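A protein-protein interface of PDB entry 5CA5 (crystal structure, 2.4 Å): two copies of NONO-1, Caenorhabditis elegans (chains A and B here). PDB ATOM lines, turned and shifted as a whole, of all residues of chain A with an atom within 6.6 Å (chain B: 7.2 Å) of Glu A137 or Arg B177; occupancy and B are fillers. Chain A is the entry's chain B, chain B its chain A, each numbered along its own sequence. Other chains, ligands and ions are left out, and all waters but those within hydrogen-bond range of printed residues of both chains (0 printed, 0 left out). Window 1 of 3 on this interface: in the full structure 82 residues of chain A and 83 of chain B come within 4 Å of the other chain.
Position printed for both chains: 98.
Of the 10 pairs that touch across the chains among the printed residues, none has its exchanged pair printed and touching as well.
Glu A137 touches one residue of chain B.
No residue of chain B comes within 4 Å of Gly A136.
Printed residues of chain A within 4 Å of Pro B176: Asp A129 and Glu A130.
Printed residues of chain B within 4 Å of Asp A129: Pro B176.
Of the printed residues of chain A, Asp B178 touches Ile A127 (3.4 Å) and Val A128 (2.8 Å).
Val A99 touches none of the printed residues of chain B.
The nearest residue of chain B that does not touch Glu A137 is Glu B179 (6.7 Å).
The nearest residue of chain A that does not touch Arg B177 is Thr A135 (4.5 Å).
The nearest printed residue of chain A that does not touch Pro B176 is Val A128 (4.7 Å).
Hydrophobic or aromatic side chains of chain B that line the printed part of chain A: Pro B176.
Along chain B the printed residues that touch a printed residue of chain A span positions 176 to 179.
Hydrophobic or aromatic side chains of chain A within 4 Å of the printed part of chain B: Val A125, Ile A127, Val A128 and Ile A139.
Among the printed residues, 10 pairs touch across the chains.
The backbone carbonyl oxygen (O) of Val A125 sits at hydrogen-bond distance from the backbone NH (N) of Ile A139 (2.8 Å).
OD1 of Asp B178 sits close to N of Asp B180.
The side-chain hydroxyl of Thr A135 is in hydrogen-bond range of the backbone carbonyl oxygen of Ile A127 (2.6 Å).
OG1 of Thr A135 sits at hydrogen-bond distance from O of Glu A137, at 3.3 Å.
N of Ile A127 lies within hydrogen-bond range of O of Glu A137, 3.0 Å away.
The backbone carbonyl oxygen of Pro B176 is in hydrogen-bond range of the backbone NH of Glu A130 (3.4 Å).
N of Asp B178 lies within hydrogen-bond range of O of Val A128 (2.8 Å).
The side-chain carboxylate of Glu A137 is in salt-bridge range of the guanidinium group of Arg B177.
Among the printed residues, pairs that only touch across the chains: Val A125 with Glu B179 (3.4 Å), Ile A127 with Asp B178 (3.4 Å), Val A128 with Arg B177 (3.6 Å), Ile A127 with Arg B177 (3.7 Å), Ile A127 with Glu B179 (3.8 Å), Asp A129 with Pro B176 (3.9 Å) and Ile A139 with Glu B179 (3.95 Å).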
ATOM      1  N   ARG A  98      15.682  30.169   0.791  1.00  0.00           N
ATOM      2  CA  ARG A  98      15.432  29.176   1.835  1.00  0.00           C
ATOM      3  C   ARG A  98      16.812  28.706   2.288  1.00  0.00           C
ATOM      4  O   ARG A  98      17.523  27.999   1.553  1.00  0.00           O
ATOM      5  CB  ARG A  98      14.591  27.988   1.343  1.00  0.00           C
ATOM      6  CG  ARG A  98      14.287  26.935   2.426  1.00  0.00           C
ATOM      7  CD  ARG A  98      13.355  25.822   1.953  1.00  0.00           C
ATOM      8  NE  ARG A  98      13.417  25.585   0.501  1.00  0.00           N
ATOM      9  CZ  ARG A  98      12.409  25.797  -0.344  1.00  0.00           C
ATOM     10  NH1 ARG A  98      11.237  26.234   0.105  1.00  0.00           N
ATOM     11  NH2 ARG A  98      12.559  25.558  -1.640  1.00  0.00           N
ATOM     12  N   VAL A  99      17.204  29.198   3.463  1.00  0.00           N
ATOM     13  CA  VAL A  99      18.429  28.879   4.171  1.00  0.00           C
ATOM     14  C   VAL A  99      18.137  27.609   5.003  1.00  0.00           C
ATOM     15  O   VAL A  99      17.042  27.453   5.572  1.00  0.00           O
ATOM     16  CB  VAL A  99      18.859  30.057   5.052  1.00  0.00           C
ATOM     17  CG1 VAL A  99      20.211  29.789   5.671  1.00  0.00           C
ATOM     18  CG2 VAL A  99      18.903  31.342   4.243  1.00  0.00           C
ATOM     19  N   LYS A 100      19.116  26.695   5.020  1.00  0.00           N
ATOM     20  CA  LYS A 100      19.024  25.404   5.689  1.00  0.00           C
ATOM     21  C   LYS A 100      20.400  25.150   6.302  1.00  0.00           C
ATOM     22  O   LYS A 100      21.332  25.903   6.010  1.00  0.00           O
ATOM     23  CB  LYS A 100      18.622  24.331   4.654  1.00  0.00           C
ATOM     24  CG  LYS A 100      18.174  22.980   5.209  1.00  0.00           C
ATOM     25  CD  LYS A 100      19.086  21.879   4.667  1.00  0.00           C
ATOM     26  CE  LYS A 100      18.584  20.474   4.899  1.00  0.00           C
ATOM     27  NZ  LYS A 100      19.547  19.469   4.359  1.00  0.00           N
ATOM     28  N   GLU A 101      20.514  24.148   7.209  1.00  0.00           N
ATOM     29  CA  GLU A 101      21.741  23.807   7.940  1.00  0.00           C
ATOM     30  C   GLU A 101      22.199  24.946   8.843  1.00  0.00           C
ATOM     31  O   GLU A 101      23.388  25.063   9.141  1.00  0.00           O
ATOM     32  CB  GLU A 101      22.872  23.351   6.978  1.00  0.00           C
ATOM     33  CG  GLU A 101      22.540  22.107   6.173  1.00  0.00           C
ATOM     34  CD  GLU A 101      22.137  20.906   6.993  1.00  0.00           C
ATOM     35  OE1 GLU A 101      22.659  20.745   8.122  1.00  0.00           O
ATOM     36  OE2 GLU A 101      21.307  20.112   6.496  1.00  0.00           O
ATOM     37  N   LEU A 102      21.248  25.811   9.257  1.00  0.00           N
ATOM     38  CA  LEU A 102      21.521  26.924  10.165  1.00  0.00           C
ATOM     39  C   LEU A 102      21.821  26.347  11.550  1.00  0.00           C
ATOM     40  O   LEU A 102      21.191  25.372  11.958  1.00  0.00           O
ATOM     41  CB  LEU A 102      20.297  27.844  10.268  1.00  0.00           C
ATOM     42  CG  LEU A 102      20.114  28.946   9.263  1.00  0.00           C
ATOM     43  CD1 LEU A 102      18.873  29.704   9.523  1.00  0.00           C
ATOM     44  CD2 LEU A 102      21.238  29.918   9.322  1.00  0.00           C
ATOM     45  N   LEU A 111      22.050  36.341  10.608  1.00  0.00           N
ATOM     46  CA  LEU A 111      21.617  35.995   9.260  1.00  0.00           C
ATOM     47  C   LEU A 111      21.431  37.257   8.422  1.00  0.00           C
ATOM     48  O   LEU A 111      21.796  37.250   7.237  1.00  0.00           O
ATOM     49  CB  LEU A 111      20.282  35.231   9.367  1.00  0.00           C
ATOM     50  CG  LEU A 111      19.850  34.349   8.203  1.00  0.00           C
ATOM     51  CD1 LEU A 111      20.866  33.250   7.931  1.00  0.00           C
ATOM     52  CD2 LEU A 111      18.445  33.748   8.481  1.00  0.00           C
ATOM     53  N   VAL A 125      15.159  35.890   8.789  1.00  0.00           N
ATOM     54  CA  VAL A 125      14.548  35.251   9.937  1.00  0.00           C
ATOM     55  C   VAL A 125      15.005  33.785  10.036  1.00  0.00           C
ATOM     56  O   VAL A 125      15.104  33.090   9.004  1.00  0.00           O
ATOM     57  CB  VAL A 125      12.993  35.461   9.923  1.00  0.00           C
ATOM     58  CG1 VAL A 125      12.327  34.804   8.706  1.00  0.00           C
ATOM     59  CG2 VAL A 125      12.351  35.030  11.216  1.00  0.00           C
ATOM     60  N   HIS A 126      15.333  33.353  11.284  1.00  0.00           N
ATOM     61  CA  HIS A 126      15.649  31.965  11.608  1.00  0.00           C
ATOM     62  C   HIS A 126      14.341  31.437  12.174  1.00  0.00           C
ATOM     63  O   HIS A 126      13.977  31.816  13.269  1.00  0.00           O
ATOM     64  CB  HIS A 126      16.795  31.817  12.676  1.00  0.00           C
ATOM     65  CG  HIS A 126      17.235  30.382  12.869  1.00  0.00           C
ATOM     66  ND1 HIS A 126      18.456  30.069  13.437  1.00  0.00           N
ATOM     67  CD2 HIS A 126      16.607  29.219  12.528  1.00  0.00           C
ATOM     68  CE1 HIS A 126      18.528  28.743  13.438  1.00  0.00           C
ATOM     69  NE2 HIS A 126      17.439  28.188  12.902  1.00  0.00           N
ATOM     70  N   ILE A 127      13.610  30.616  11.416  1.00  0.00           N
ATOM     71  CA  ILE A 127      12.309  30.032  11.810  1.00  0.00           C
ATOM     72  C   ILE A 127      12.463  29.140  13.051  1.00  0.00           C
ATOM     73  O   ILE A 127      13.472  28.410  13.205  1.00  0.00           O
ATOM     74  CB  ILE A 127      11.664  29.283  10.618  1.00  0.00           C
ATOM     75  CG1 ILE A 127      11.549  30.203   9.385  1.00  0.00           C
ATOM     76  CG2 ILE A 127      10.294  28.683  10.966  1.00  0.00           C
ATOM     77  CD1 ILE A 127      11.690  29.477   8.064  1.00  0.00           C
ATOM     78  N   VAL A 128      11.482  29.277  13.981  1.00  0.00           N
ATOM     79  CA  VAL A 128      11.387  28.488  15.214  1.00  0.00           C
ATOM     80  C   VAL A 128      10.056  27.717  15.248  1.00  0.00           C
ATOM     81  O   VAL A 128       9.101  28.085  14.535  1.00  0.00           O
ATOM     82  CB  VAL A 128      11.689  29.263  16.520  1.00  0.00           C
ATOM     83  CG1 VAL A 128      13.106  29.829  16.506  1.00  0.00           C
ATOM     84  CG2 VAL A 128      10.659  30.358  16.791  1.00  0.00           C
ATOM     85  N   ASP A 129      10.014  26.608  16.019  1.00  0.00           N
ATOM     86  CA  ASP A 129       8.806  25.797  16.179  1.00  0.00           C
ATOM     87  C   ASP A 129       7.858  26.454  17.204  1.00  0.00           C
ATOM     88  O   ASP A 129       8.128  27.585  17.638  1.00  0.00           O
ATOM     89  CB  ASP A 129       9.155  24.333  16.540  1.00  0.00           C
ATOM     90  CG  ASP A 129      10.243  24.109  17.573  1.00  0.00           C
ATOM     91  OD1 ASP A 129      10.197  24.763  18.638  1.00  0.00           O
ATOM     92  OD2 ASP A 129      11.112  23.233  17.340  1.00  0.00           O
ATOM     93  N   GLU A 130       6.741  25.768  17.573  1.00  0.00           N
ATOM     94  CA  GLU A 130       5.755  26.273  18.543  1.00  0.00           C
ATOM     95  C   GLU A 130       6.442  26.482  19.894  1.00  0.00           C
ATOM     96  O   GLU A 130       6.240  27.517  20.549  1.00  0.00           O
ATOM     97  CB  GLU A 130       4.569  25.301  18.684  1.00  0.00           C
ATOM     98  CG  GLU A 130       3.424  25.840  19.534  1.00  0.00           C
ATOM     99  CD  GLU A 130       2.293  24.873  19.837  1.00  0.00           C
ATOM    100  OE1 GLU A 130       1.978  24.017  18.977  1.00  0.00           O
ATOM    101  OE2 GLU A 130       1.698  25.000  20.932  1.00  0.00           O
ATOM    102  N   PRO A 134      14.949  26.778  17.581  1.00  0.00           N
ATOM    103  CA  PRO A 134      15.375  26.943  16.181  1.00  0.00           C
ATOM    104  C   PRO A 134      15.158  25.669  15.357  1.00  0.00           C
ATOM    105  O   PRO A 134      15.276  24.549  15.880  1.00  0.00           O
ATOM    106  CB  PRO A 134      16.857  27.306  16.300  1.00  0.00           C
ATOM    107  CG  PRO A 134      17.263  26.829  17.659  1.00  0.00           C
ATOM    108  CD  PRO A 134      16.074  27.035  18.508  1.00  0.00           C
ATOM    109  N   THR A 135      14.790  25.852  14.077  1.00  0.00           N
ATOM    110  CA  THR A 135      14.475  24.751  13.165  1.00  0.00           C
ATOM    111  C   THR A 135      15.646  24.361  12.277  1.00  0.00           C
ATOM    112  O   THR A 135      15.615  23.293  11.677  1.00  0.00           O
ATOM    113  CB  THR A 135      13.241  25.124  12.330  1.00  0.00           C
ATOM    114  OG1 THR A 135      13.491  26.339  11.612  1.00  0.00           O
ATOM    115  CG2 THR A 135      11.983  25.282  13.177  1.00  0.00           C
ATOM    116  N   GLY A 136      16.667  25.224  12.214  1.00  0.00           N
ATOM    117  CA  GLY A 136      17.828  25.048  11.344  1.00  0.00           C
ATOM    118  C   GLY A 136      17.539  25.593   9.948  1.00  0.00           C
ATOM    119  O   GLY A 136      18.412  25.617   9.087  1.00  0.00           O
ATOM    120  N   GLU A 137      16.292  26.022   9.723  1.00  0.00           N
ATOM    121  CA  GLU A 137      15.807  26.617   8.495  1.00  0.00           C
ATOM    122  C   GLU A 137      15.572  28.119   8.700  1.00  0.00           C
ATOM    123  O   GLU A 137      15.129  28.556   9.762  1.00  0.00           O
ATOM    124  CB  GLU A 137      14.486  25.957   8.064  1.00  0.00           C
ATOM    125  CG  GLU A 137      14.651  24.632   7.329  1.00  0.00           C
ATOM    126  CD  GLU A 137      13.610  24.334   6.260  1.00  0.00           C
ATOM    127  OE1 GLU A 137      12.924  25.275   5.792  1.00  0.00           O
ATOM    128  OE2 GLU A 137      13.520  23.154   5.853  1.00  0.00           O
ATOM    129  N   GLY A 138      15.818  28.887   7.656  1.00  0.00           N
ATOM    130  CA  GLY A 138      15.608  30.327   7.690  1.00  0.00           C
ATOM    131  C   GLY A 138      15.134  30.899   6.375  1.00  0.00           C
ATOM    132  O   GLY A 138      15.180  30.210   5.352  1.00  0.00           O
ATOM    133  N   ILE A 139      14.687  32.179   6.398  1.00  0.00           N
ATOM    134  CA  ILE A 139      14.231  32.927   5.205  1.00  0.00           C
ATOM    135  C   ILE A 139      15.062  34.180   5.067  1.00  0.00           C
ATOM    136  O   ILE A 139      15.221  34.909   6.037  1.00  0.00           O
ATOM    137  CB  ILE A 139      12.689  33.287   5.199  1.00  0.00           C
ATOM    138  CG1 ILE A 139      11.789  32.039   5.238  1.00  0.00           C
ATOM    139  CG2 ILE A 139      12.288  34.192   3.974  1.00  0.00           C
ATOM    140  CD1 ILE A 139      10.414  32.311   5.774  1.00  0.00           C
ATOM    141  N   ARG B  98      -3.278  19.286   9.407  1.00  0.00           N
ATOM    142  CA  ARG B  98      -2.471  19.208   8.195  1.00  0.00           C
ATOM    143  C   ARG B  98      -2.962  17.963   7.475  1.00  0.00           C
ATOM    144  O   ARG B  98      -2.747  16.831   7.951  1.00  0.00           O
ATOM    145  CB  ARG B  98      -0.960  19.113   8.475  1.00  0.00           C
ATOM    146  CG  ARG B  98      -0.121  19.252   7.200  1.00  0.00           C
ATOM    147  CD  ARG B  98       1.382  19.234   7.427  1.00  0.00           C
ATOM    148  NE  ARG B  98       1.877  20.501   7.964  1.00  0.00           N
ATOM    149  CZ  ARG B  98       2.166  20.712   9.245  1.00  0.00           C
ATOM    150  NH1 ARG B  98       2.015  19.738  10.137  1.00  0.00           N
ATOM    151  NH2 ARG B  98       2.606  21.897   9.646  1.00  0.00           N
ATOM    152  N   LEU B 174      -1.318  20.333  12.915  1.00  0.00           N
ATOM    153  CA  LEU B 174      -0.638  21.379  12.170  1.00  0.00           C
ATOM    154  C   LEU B 174       0.147  22.203  13.185  1.00  0.00           C
ATOM    155  O   LEU B 174      -0.385  23.172  13.758  1.00  0.00           O
ATOM    156  CB  LEU B 174      -1.645  22.225  11.381  1.00  0.00           C
ATOM    157  CG  LEU B 174      -1.103  23.155  10.286  1.00  0.00           C
ATOM    158  CD1 LEU B 174      -1.842  22.944   9.007  1.00  0.00           C
ATOM    159  CD2 LEU B 174      -1.176  24.561  10.736  1.00  0.00           C
ATOM    160  N   GLU B 175       1.394  21.750  13.461  1.00  0.00           N
ATOM    161  CA  GLU B 175       2.309  22.413  14.387  1.00  0.00           C
ATOM    162  C   GLU B 175       2.710  23.778  13.790  1.00  0.00           C
ATOM    163  O   GLU B 175       3.246  23.828  12.676  1.00  0.00           O
ATOM    164  CB  GLU B 175       3.547  21.533  14.716  1.00  0.00           C
ATOM    165  CG  GLU B 175       3.247  20.112  15.187  1.00  0.00           C
ATOM    166  CD  GLU B 175       2.891  19.890  16.654  1.00  0.00           C
ATOM    167  OE1 GLU B 175       3.636  19.156  17.342  1.00  0.00           O
ATOM    168  OE2 GLU B 175       1.827  20.389  17.093  1.00  0.00           O
ATOM    169  N   PRO B 176       2.323  24.900  14.442  1.00  0.00           N
ATOM    170  CA  PRO B 176       2.640  26.214  13.854  1.00  0.00           C
ATOM    171  C   PRO B 176       4.130  26.543  13.875  1.00  0.00           C
ATOM    172  O   PRO B 176       4.841  26.156  14.786  1.00  0.00           O
ATOM    173  CB  PRO B 176       1.799  27.195  14.685  1.00  0.00           C
ATOM    174  CG  PRO B 176       1.571  26.497  15.993  1.00  0.00           C
ATOM    175  CD  PRO B 176       1.606  25.029  15.737  1.00  0.00           C
ATOM    176  N   ARG B 177       4.600  27.226  12.846  1.00  0.00           N
ATOM    177  CA  ARG B 177       5.995  27.642  12.714  1.00  0.00           C
ATOM    178  C   ARG B 177       6.097  29.165  12.777  1.00  0.00           C
ATOM    179  O   ARG B 177       5.317  29.874  12.140  1.00  0.00           O
ATOM    180  CB  ARG B 177       6.611  27.117  11.408  1.00  0.00           C
ATOM    181  CG  ARG B 177       7.216  25.721  11.496  1.00  0.00           C
ATOM    182  CD  ARG B 177       8.354  25.582  10.512  1.00  0.00           C
ATOM    183  NE  ARG B 177       8.166  24.532   9.516  1.00  0.00           N
ATOM    184  CZ  ARG B 177       8.862  24.450   8.381  1.00  0.00           C
ATOM    185  NH1 ARG B 177       9.766  25.378   8.076  1.00  0.00           N
ATOM    186  NH2 ARG B 177       8.634  23.461   7.526  1.00  0.00           N
ATOM    187  N   ASP B 178       7.045  29.669  13.566  1.00  0.00           N
ATOM    188  CA  ASP B 178       7.251  31.111  13.705  1.00  0.00           C
ATOM    189  C   ASP B 178       8.289  31.674  12.667  1.00  0.00           C
ATOM    190  O   ASP B 178       9.515  31.683  12.897  1.00  0.00           O
ATOM    191  CB  ASP B 178       7.570  31.458  15.170  1.00  0.00           C
ATOM    192  CG  ASP B 178       7.943  32.893  15.436  1.00  0.00           C
ATOM    193  OD1 ASP B 178       7.457  33.779  14.704  1.00  0.00           O
ATOM    194  OD2 ASP B 178       8.696  33.132  16.386  1.00  0.00           O
ATOM    195  N   GLU B 179       7.752  32.107  11.515  1.00  0.00           N
ATOM    196  CA  GLU B 179       8.480  32.677  10.381  1.00  0.00           C
ATOM    197  C   GLU B 179       8.456  34.171  10.474  1.00  0.00           C
ATOM    198  O   GLU B 179       9.042  34.853   9.632  1.00  0.00           O
ATOM    199  CB  GLU B 179       7.803  32.276   9.057  1.00  0.00           C
ATOM    200  CG  GLU B 179       7.853  30.789   8.769  1.00  0.00           C
ATOM    201  CD  GLU B 179       7.362  30.387   7.392  1.00  0.00           C
ATOM    202  OE1 GLU B 179       7.709  29.265   6.958  1.00  0.00           O
ATOM    203  OE2 GLU B 179       6.634  31.183   6.751  1.00  0.00           O
ATOM    204  N   ASP B 180       7.752  34.688  11.484  1.00  0.00           N
ATOM    205  CA  ASP B 180       7.573  36.120  11.694  1.00  0.00           C
ATOM    206  C   ASP B 180       8.530  36.731  12.691  1.00  0.00           C
ATOM    207  O   ASP B 180       9.165  37.725  12.369  1.00  0.00           O
ATOM    208  CB  ASP B 180       6.098  36.441  12.001  1.00  0.00           C
ATOM    209  CG  ASP B 180       5.181  36.071  10.841  1.00  0.00           C
ATOM    210  OD1 ASP B 180       5.428  36.558   9.706  1.00  0.00           O
ATOM    211  OD2 ASP B 180       4.241  35.269  11.057  1.00  0.00           O
